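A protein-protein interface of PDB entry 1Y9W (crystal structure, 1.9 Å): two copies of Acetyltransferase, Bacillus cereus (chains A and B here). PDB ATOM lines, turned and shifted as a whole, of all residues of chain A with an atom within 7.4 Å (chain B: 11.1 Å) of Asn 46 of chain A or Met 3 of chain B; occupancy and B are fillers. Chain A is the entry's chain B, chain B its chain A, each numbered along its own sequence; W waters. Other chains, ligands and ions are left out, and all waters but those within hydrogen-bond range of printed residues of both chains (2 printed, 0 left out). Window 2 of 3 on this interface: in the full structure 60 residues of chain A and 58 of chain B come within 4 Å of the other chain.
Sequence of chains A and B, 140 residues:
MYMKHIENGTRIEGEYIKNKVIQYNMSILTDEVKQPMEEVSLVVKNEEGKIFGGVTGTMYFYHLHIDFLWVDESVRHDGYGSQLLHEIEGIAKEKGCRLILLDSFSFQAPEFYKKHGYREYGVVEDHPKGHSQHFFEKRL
Of the 9 printed residues of chain B, 7 touch a printed residue of chain A.
Of the 10 printed residues of chain A, 7 touch a printed residue of chain B.
Among the printed residues, 11 pairs touch across the chains.
Among the printed residues, Asp or Glu carboxylates within 4 Å of a Lys or Arg side-chain nitrogen of the other chain: Lys 45 of chain A with Glu 7 of chain B (3.0 Å) and Lys 45 of chain A with Glu 13 of chain B (2.6 Å).
Of chain B, only Met 3 comes within 4 Å of Asn 46 of chain A.
Of chain A, only Asn 46 (3.8 Å) and Glu 47 (3.8 Å) come within 4 Å of Met 3 of chain B.
Glu 47 of chain A touches just one residue of chain B: Met 3 (3.8 Å).
No residue of chain B comes within 4 Å of Glu 48 of chain A.
No residue of chain B comes within 4 Å of Lys 50 of chain A.
Of the printed residues of chain A, Ile 6 of chain B touches Val 44.
Printed residues of chain B within 4 Å of Val 44 of chain A: His 5 and Ile 6.
Of the printed residues of chain A, His 5 of chain B touches Val 44 and Lys 45.
Of the printed residues of chain A, Tyr 16 of chain B touches Ile 51 (3.6 Å).
Met 1 of chain B touches none of the printed residues of chain A.
The backbone carbonyl oxygen of Val 44 of chain A lies within hydrogen-bond range of the backbone NH of Phe 52 of chain A, 3.3 Å away.
OE1 of Glu 48 of chain A lies close to OD1 of Asn 46 of chain A.
NE2 of His 5 of chain B is in hydrogen-bond range of OE1 of Glu 7 of chain B (3.3 Å).
Water W2 lies within hydrogen-bond range of the side-chain amino group of Lys 4 of chain B and the side-chain amide nitrogen of Asn 46 of chain A.
Water W1 lies within hydrogen-bond range of OE1 of Glu 13 of chain B (2.8 Å), OE2 of Glu 7 of chain B (2.8 Å) and NZ of Lys 45 of chain A (3.1 Å).
No position is printed for both chains.
Val 44 of chain A touches His 5 of chain B (CA to O, 3.0 Å).
Val 44 of chain A touches Ile 6 of chain B.
Lys 45 of chain A touches Lys 4 of chain B.
O of Met 3 of chain B touches ND2 of Asn 46 of chain A, 3.8 Å away.
Glu 47 of chain A touches Met 3 of chain B (N to O, 3.8 Å).
Ile 51 of chain A touches Tyr 16 of chain B.
Phe 52 of chain A touches Lys 4 of chain B.
Lys 4 of chain B touches Tyr 80 of chain A (CD to OH, 3.1 Å).
The side-chain carboxylate of Glu 7 of chain B lies within salt-bridge range of the side-chain amino group of Lys 45 of chain A (3.0 Å).
The side-chain amino group (NZ) of Lys 45 of chain A lies within salt-bridge range of the side-chain carboxylate (OE2) of Glu 13 of chain B, at 2.6 Å.
The backbone carbonyl oxygen (O) of His 5 of chain B sits at hydrogen-bond distance from the backbone NH (N) of Lys 45 of chain A.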
ATOM      1  N   VAL A  44     -18.430 -31.985 -17.702  1.00  0.00           N
ATOM      2  CA  VAL A  44     -17.363 -31.873 -16.725  1.00  0.00           C
ATOM      3  C   VAL A  44     -16.272 -31.043 -17.410  1.00  0.00           C
ATOM      4  O   VAL A  44     -15.772 -31.399 -18.483  1.00  0.00           O
ATOM      5  CB  VAL A  44     -16.828 -33.257 -16.310  1.00  0.00           C
ATOM      6  CG1 VAL A  44     -16.209 -33.963 -17.502  1.00  0.00           C
ATOM      7  CG2 VAL A  44     -15.823 -33.097 -15.180  1.00  0.00           C
ATOM      8  N   LYS A  45     -15.925 -29.917 -16.798  1.00  0.00           N
ATOM      9  CA  LYS A  45     -14.930 -29.029 -17.379  1.00  0.00           C
ATOM     10  C   LYS A  45     -13.639 -28.831 -16.605  1.00  0.00           C
ATOM     11  O   LYS A  45     -13.545 -29.074 -15.398  1.00  0.00           O
ATOM     12  CB  LYS A  45     -15.552 -27.659 -17.660  1.00  0.00           C
ATOM     13  CG  LYS A  45     -16.550 -27.665 -18.793  1.00  0.00           C
ATOM     14  CD  LYS A  45     -17.087 -26.269 -19.050  1.00  0.00           C
ATOM     15  CE  LYS A  45     -17.961 -26.246 -20.291  1.00  0.00           C
ATOM     16  NZ  LYS A  45     -18.467 -24.879 -20.601  1.00  0.00           N
ATOM     17  N   ASN A  46     -12.646 -28.373 -17.350  1.00  0.00           N
ATOM     18  CA  ASN A  46     -11.325 -28.093 -16.839  1.00  0.00           C
ATOM     19  C   ASN A  46     -11.345 -26.668 -16.316  1.00  0.00           C
ATOM     20  O   ASN A  46     -12.309 -25.932 -16.539  1.00  0.00           O
ATOM     21  CB  ASN A  46     -10.325 -28.189 -17.976  1.00  0.00           C
ATOM     22  CG  ASN A  46      -8.915 -28.215 -17.494  1.00  0.00           C
ATOM     23  OD1 ASN A  46      -7.977 -28.167 -18.290  1.00  0.00           O
ATOM     24  ND2 ASN A  46      -8.742 -28.303 -16.177  1.00  0.00           N
ATOM     25  N   GLU A  47     -10.283 -26.277 -15.625  1.00  0.00           N
ATOM     26  CA  GLU A  47     -10.188 -24.924 -15.098  1.00  0.00           C
ATOM     27  C   GLU A  47     -10.247 -23.962 -16.291  1.00  0.00           C
ATOM     28  O   GLU A  47     -10.771 -22.852 -16.193  1.00  0.00           O
ATOM     29  CB  GLU A  47      -8.866 -24.749 -14.339  1.00  0.00           C
ATOM     30  CG  GLU A  47      -8.740 -23.430 -13.576  1.00  0.00           C
ATOM     31  CD  GLU A  47      -9.648 -23.359 -12.352  1.00  0.00           C
ATOM     32  OE1 GLU A  47      -9.715 -22.281 -11.718  1.00  0.00           O
ATOM     33  OE2 GLU A  47     -10.288 -24.382 -12.020  1.00  0.00           O
ATOM     34  N   GLU A  48      -9.723 -24.412 -17.426  1.00  0.00           N
ATOM     35  CA  GLU A  48      -9.696 -23.609 -18.646  1.00  0.00           C
ATOM     36  C   GLU A  48     -10.995 -23.748 -19.440  1.00  0.00           C
ATOM     37  O   GLU A  48     -11.102 -23.233 -20.555  1.00  0.00           O
ATOM     38  CB  GLU A  48      -8.531 -24.055 -19.526  1.00  0.00           C
ATOM     39  CG  GLU A  48      -7.330 -24.548 -18.737  1.00  0.00           C
ATOM     40  CD  GLU A  48      -6.443 -25.473 -19.550  1.00  0.00           C
ATOM     41  OE1 GLU A  48      -6.973 -26.447 -20.139  1.00  0.00           O
ATOM     42  OE2 GLU A  48      -5.217 -25.229 -19.590  1.00  0.00           O
ATOM     43  N   GLY A  49     -11.973 -24.449 -18.872  1.00  0.00           N
ATOM     44  CA  GLY A  49     -13.236 -24.641 -19.563  1.00  0.00           C
ATOM     45  C   GLY A  49     -13.128 -25.710 -20.635  1.00  0.00           C
ATOM     46  O   GLY A  49     -13.890 -25.720 -21.606  1.00  0.00           O
ATOM     47  N   LYS A  50     -12.160 -26.605 -20.464  1.00  0.00           N
ATOM     48  CA  LYS A  50     -11.946 -27.699 -21.401  1.00  0.00           C
ATOM     49  C   LYS A  50     -12.880 -28.812 -20.947  1.00  0.00           C
ATOM     50  O   LYS A  50     -12.997 -29.078 -19.754  1.00  0.00           O
ATOM     51  CB  LYS A  50     -10.496 -28.178 -21.322  1.00  0.00           C
ATOM     52  CG  LYS A  50     -10.016 -28.929 -22.545  1.00  0.00           C
ATOM     53  CD  LYS A  50     -10.855 -30.158 -22.831  1.00  0.00           C
ATOM     54  CE  LYS A  50     -10.415 -30.815 -24.127  1.00  0.00           C
ATOM     55  NZ  LYS A  50      -8.961 -31.147 -24.090  1.00  0.00           N
ATOM     56  N   ILE A  51     -13.547 -29.465 -21.888  1.00  0.00           N
ATOM     57  CA  ILE A  51     -14.470 -30.532 -21.529  1.00  0.00           C
ATOM     58  C   ILE A  51     -13.965 -31.939 -21.856  1.00  0.00           C
ATOM     59  O   ILE A  51     -13.566 -32.217 -22.983  1.00  0.00           O
ATOM     60  CB  ILE A  51     -15.843 -30.306 -22.209  1.00  0.00           C
ATOM     61  CG1 ILE A  51     -16.638 -31.613 -22.228  1.00  0.00           C
ATOM     62  CG2 ILE A  51     -15.651 -29.756 -23.607  1.00  0.00           C
ATOM     63  CD1 ILE A  51     -17.971 -31.499 -22.914  1.00  0.00           C
ATOM     64  N   PHE A  52     -13.976 -32.822 -20.857  1.00  0.00           N
ATOM     65  CA  PHE A  52     -13.545 -34.201 -21.063  1.00  0.00           C
ATOM     66  C   PHE A  52     -14.672 -35.180 -20.784  1.00  0.00           C
ATOM     67  O   PHE A  52     -14.441 -36.382 -20.657  1.00  0.00           O
ATOM     68  CB  PHE A  52     -12.349 -34.573 -20.180  1.00  0.00           C
ATOM     69  CG  PHE A  52     -11.838 -33.457 -19.335  1.00  0.00           C
ATOM     70  CD1 PHE A  52     -12.600 -32.962 -18.280  1.00  0.00           C
ATOM     71  CD2 PHE A  52     -10.590 -32.891 -19.594  1.00  0.00           C
ATOM     72  CE1 PHE A  52     -12.128 -31.914 -17.490  1.00  0.00           C
ATOM     73  CE2 PHE A  52     -10.104 -31.842 -18.814  1.00  0.00           C
ATOM     74  CZ  PHE A  52     -10.875 -31.350 -17.758  1.00  0.00           C
ATOM     75  N   TYR A  80     -15.763 -40.095 -13.755  1.00  0.00           N
ATOM     76  CA  TYR A  80     -16.590 -38.953 -14.114  1.00  0.00           C
ATOM     77  C   TYR A  80     -17.933 -39.452 -14.632  1.00  0.00           C
ATOM     78  O   TYR A  80     -18.949 -38.759 -14.536  1.00  0.00           O
ATOM     79  CB  TYR A  80     -15.891 -38.115 -15.176  1.00  0.00           C
ATOM     80  CG  TYR A  80     -14.658 -37.437 -14.643  1.00  0.00           C
ATOM     81  CD1 TYR A  80     -14.751 -36.510 -13.607  1.00  0.00           C
ATOM     82  CD2 TYR A  80     -13.396 -37.743 -15.143  1.00  0.00           C
ATOM     83  CE1 TYR A  80     -13.620 -35.909 -13.081  1.00  0.00           C
ATOM     84  CE2 TYR A  80     -12.259 -37.146 -14.623  1.00  0.00           C
ATOM     85  CZ  TYR A  80     -12.376 -36.233 -13.592  1.00  0.00           C
ATOM     86  OH  TYR A  80     -11.247 -35.655 -13.054  1.00  0.00           O
ATOM     87  N   MET B   1      -4.968 -27.381  -8.740  1.00  0.00           N
ATOM     88  CA  MET B   1      -4.246 -26.945  -9.972  1.00  0.00           C
ATOM     89  C   MET B   1      -4.576 -27.814 -11.189  1.00  0.00           C
ATOM     90  O   MET B   1      -4.086 -27.565 -12.295  1.00  0.00           O
ATOM     91  CB  MET B   1      -2.727 -26.948  -9.727  1.00  0.00           C
ATOM     92  CG  MET B   1      -1.892 -26.529 -10.944  1.00  0.00           C
ATOM     93  SD  MET B   1      -0.130 -26.334 -10.605  1.00  0.00           S
ATOM     94  CE  MET B   1       0.310 -28.011 -10.101  1.00  0.00           C
ATOM     95  N   TYR B   2      -5.411 -28.829 -10.991  1.00  0.00           N
ATOM     96  CA  TYR B   2      -5.800 -29.719 -12.085  1.00  0.00           C
ATOM     97  C   TYR B   2      -7.248 -30.169 -11.943  1.00  0.00           C
ATOM     98  O   TYR B   2      -7.703 -31.057 -12.664  1.00  0.00           O
ATOM     99  CB  TYR B   2      -4.882 -30.950 -12.118  1.00  0.00           C
ATOM    100  CG  TYR B   2      -3.460 -30.642 -12.527  1.00  0.00           C
ATOM    101  CD1 TYR B   2      -3.185 -30.074 -13.772  1.00  0.00           C
ATOM    102  CD2 TYR B   2      -2.390 -30.908 -11.669  1.00  0.00           C
ATOM    103  CE1 TYR B   2      -1.884 -29.771 -14.158  1.00  0.00           C
ATOM    104  CE2 TYR B   2      -1.080 -30.610 -12.044  1.00  0.00           C
ATOM    105  CZ  TYR B   2      -0.833 -30.039 -13.293  1.00  0.00           C
ATOM    106  OH  TYR B   2       0.454 -29.730 -13.681  1.00  0.00           O
ATOM    107  N   MET B   3      -7.973 -29.536 -11.026  1.00  0.00           N
ATOM    108  CA  MET B   3      -9.362 -29.895 -10.768  1.00  0.00           C
ATOM    109  C   MET B   3     -10.351 -29.646 -11.906  1.00  0.00           C
ATOM    110  O   MET B   3     -10.180 -28.743 -12.736  1.00  0.00           O
ATOM    111  CB  MET B   3      -9.858 -29.216  -9.481  1.00  0.00           C
ATOM    112  CG  MET B   3      -9.767 -27.695  -9.462  1.00  0.00           C
ATOM    113  SD  MET B   3     -10.021 -27.022  -7.788  1.00  0.00           S
ATOM    114  CE  MET B   3     -11.797 -27.337  -7.553  1.00  0.00           C
ATOM    115  N   LYS B   4     -11.386 -30.483 -11.920  1.00  0.00           N
ATOM    116  CA  LYS B   4     -12.442 -30.438 -12.916  1.00  0.00           C
ATOM    117  C   LYS B   4     -13.768 -30.559 -12.167  1.00  0.00           C
ATOM    118  O   LYS B   4     -13.876 -31.316 -11.202  1.00  0.00           O
ATOM    119  CB  LYS B   4     -12.279 -31.613 -13.875  1.00  0.00           C
ATOM    120  CG  LYS B   4     -10.842 -31.849 -14.287  1.00  0.00           C
ATOM    121  CD  LYS B   4     -10.674 -33.208 -14.938  1.00  0.00           C
ATOM    122  CE  LYS B   4      -9.206 -33.535 -15.170  1.00  0.00           C
ATOM    123  NZ  LYS B   4      -8.532 -32.529 -16.037  1.00  0.00           N
ATOM    124  N   HIS B   5     -14.770 -29.809 -12.608  1.00  0.00           N
ATOM    125  CA  HIS B   5     -16.081 -29.834 -11.973  1.00  0.00           C
ATOM    126  C   HIS B   5     -17.153 -30.101 -13.018  1.00  0.00           C
ATOM    127  O   HIS B   5     -16.856 -30.235 -14.205  1.00  0.00           O
ATOM    128  CB  HIS B   5     -16.354 -28.495 -11.296  1.00  0.00           C
ATOM    129  CG  HIS B   5     -16.170 -27.323 -12.206  1.00  0.00           C
ATOM    130  ND1 HIS B   5     -14.950 -27.001 -12.764  1.00  0.00           N
ATOM    131  CD2 HIS B   5     -17.056 -26.422 -12.694  1.00  0.00           C
ATOM    132  CE1 HIS B   5     -15.095 -25.955 -13.558  1.00  0.00           C
ATOM    133  NE2 HIS B   5     -16.362 -25.584 -13.534  1.00  0.00           N
ATOM    134  N   ILE B   6     -18.402 -30.174 -12.572  1.00  0.00           N
ATOM    135  CA  ILE B   6     -19.511 -30.427 -13.483  1.00  0.00           C
ATOM    136  C   ILE B   6     -20.487 -29.260 -13.480  1.00  0.00           C
ATOM    137  O   ILE B   6     -20.822 -28.718 -12.425  1.00  0.00           O
ATOM    138  CB  ILE B   6     -20.282 -31.725 -13.100  1.00  0.00           C
ATOM    139  CG1 ILE B   6     -19.369 -32.943 -13.250  1.00  0.00           C
ATOM    140  CG2 ILE B   6     -21.505 -31.897 -13.989  1.00  0.00           C
ATOM    141  CD1 ILE B   6     -20.049 -34.257 -12.920  1.00  0.00           C
ATOM    142  N   GLU B   7     -20.937 -28.879 -14.670  1.00  0.00           N
ATOM    143  CA  GLU B   7     -21.885 -27.786 -14.818  1.00  0.00           C
ATOM    144  C   GLU B   7     -22.888 -28.126 -15.910  1.00  0.00           C
ATOM    145  O   GLU B   7     -22.670 -29.049 -16.698  1.00  0.00           O
ATOM    146  CB  GLU B   7     -21.149 -26.493 -15.173  1.00  0.00           C
ATOM    147  CG  GLU B   7     -20.247 -26.611 -16.392  1.00  0.00           C
ATOM    148  CD  GLU B   7     -19.455 -25.342 -16.660  1.00  0.00           C
ATOM    149  OE1 GLU B   7     -18.761 -24.869 -15.732  1.00  0.00           O
ATOM    150  OE2 GLU B   7     -19.522 -24.819 -17.796  1.00  0.00           O
ATOM    151  N   GLU B  13     -22.986 -27.619 -26.567  1.00  0.00           N
ATOM    152  CA  GLU B  13     -22.176 -28.562 -25.810  1.00  0.00           C
ATOM    153  C   GLU B  13     -22.831 -29.942 -25.791  1.00  0.00           C
ATOM    154  O   GLU B  13     -22.146 -30.964 -25.811  1.00  0.00           O
ATOM    155  CB  GLU B  13     -21.949 -28.037 -24.394  1.00  0.00           C
ATOM    156  CG  GLU B  13     -21.186 -26.715 -24.367  1.00  0.00           C
ATOM    157  CD  GLU B  13     -21.016 -26.144 -22.967  1.00  0.00           C
ATOM    158  OE1 GLU B  13     -22.007 -26.120 -22.201  1.00  0.00           O
ATOM    159  OE2 GLU B  13     -19.893 -25.701 -22.638  1.00  0.00           O
ATOM    160  N   TYR B  16     -22.003 -31.552 -28.875  1.00  0.00           N
ATOM    161  CA  TYR B  16     -20.595 -31.940 -28.873  1.00  0.00           C
ATOM    162  C   TYR B  16     -20.456 -33.307 -28.216  1.00  0.00           C
ATOM    163  O   TYR B  16     -19.742 -34.177 -28.717  1.00  0.00           O
ATOM    164  CB  TYR B  16     -19.768 -30.910 -28.103  1.00  0.00           C
ATOM    165  CG  TYR B  16     -18.307 -31.272 -27.924  1.00  0.00           C
ATOM    166  CD1 TYR B  16     -17.470 -31.461 -29.027  1.00  0.00           C
ATOM    167  CD2 TYR B  16     -17.754 -31.405 -26.647  1.00  0.00           C
ATOM    168  CE1 TYR B  16     -16.107 -31.772 -28.861  1.00  0.00           C
ATOM    169  CE2 TYR B  16     -16.400 -31.717 -26.472  1.00  0.00           C
ATOM    170  CZ  TYR B  16     -15.584 -31.898 -27.583  1.00  0.00           C
ATOM    171  OH  TYR B  16     -14.250 -32.202 -27.413  1.00  0.00           O
HETATM  172  O   HOH W   1     -21.488 -24.802 -19.823  1.00  0.00           O
HETATM  173  O   HOH W   2      -6.671 -30.627 -16.016  1.00  0.00           O
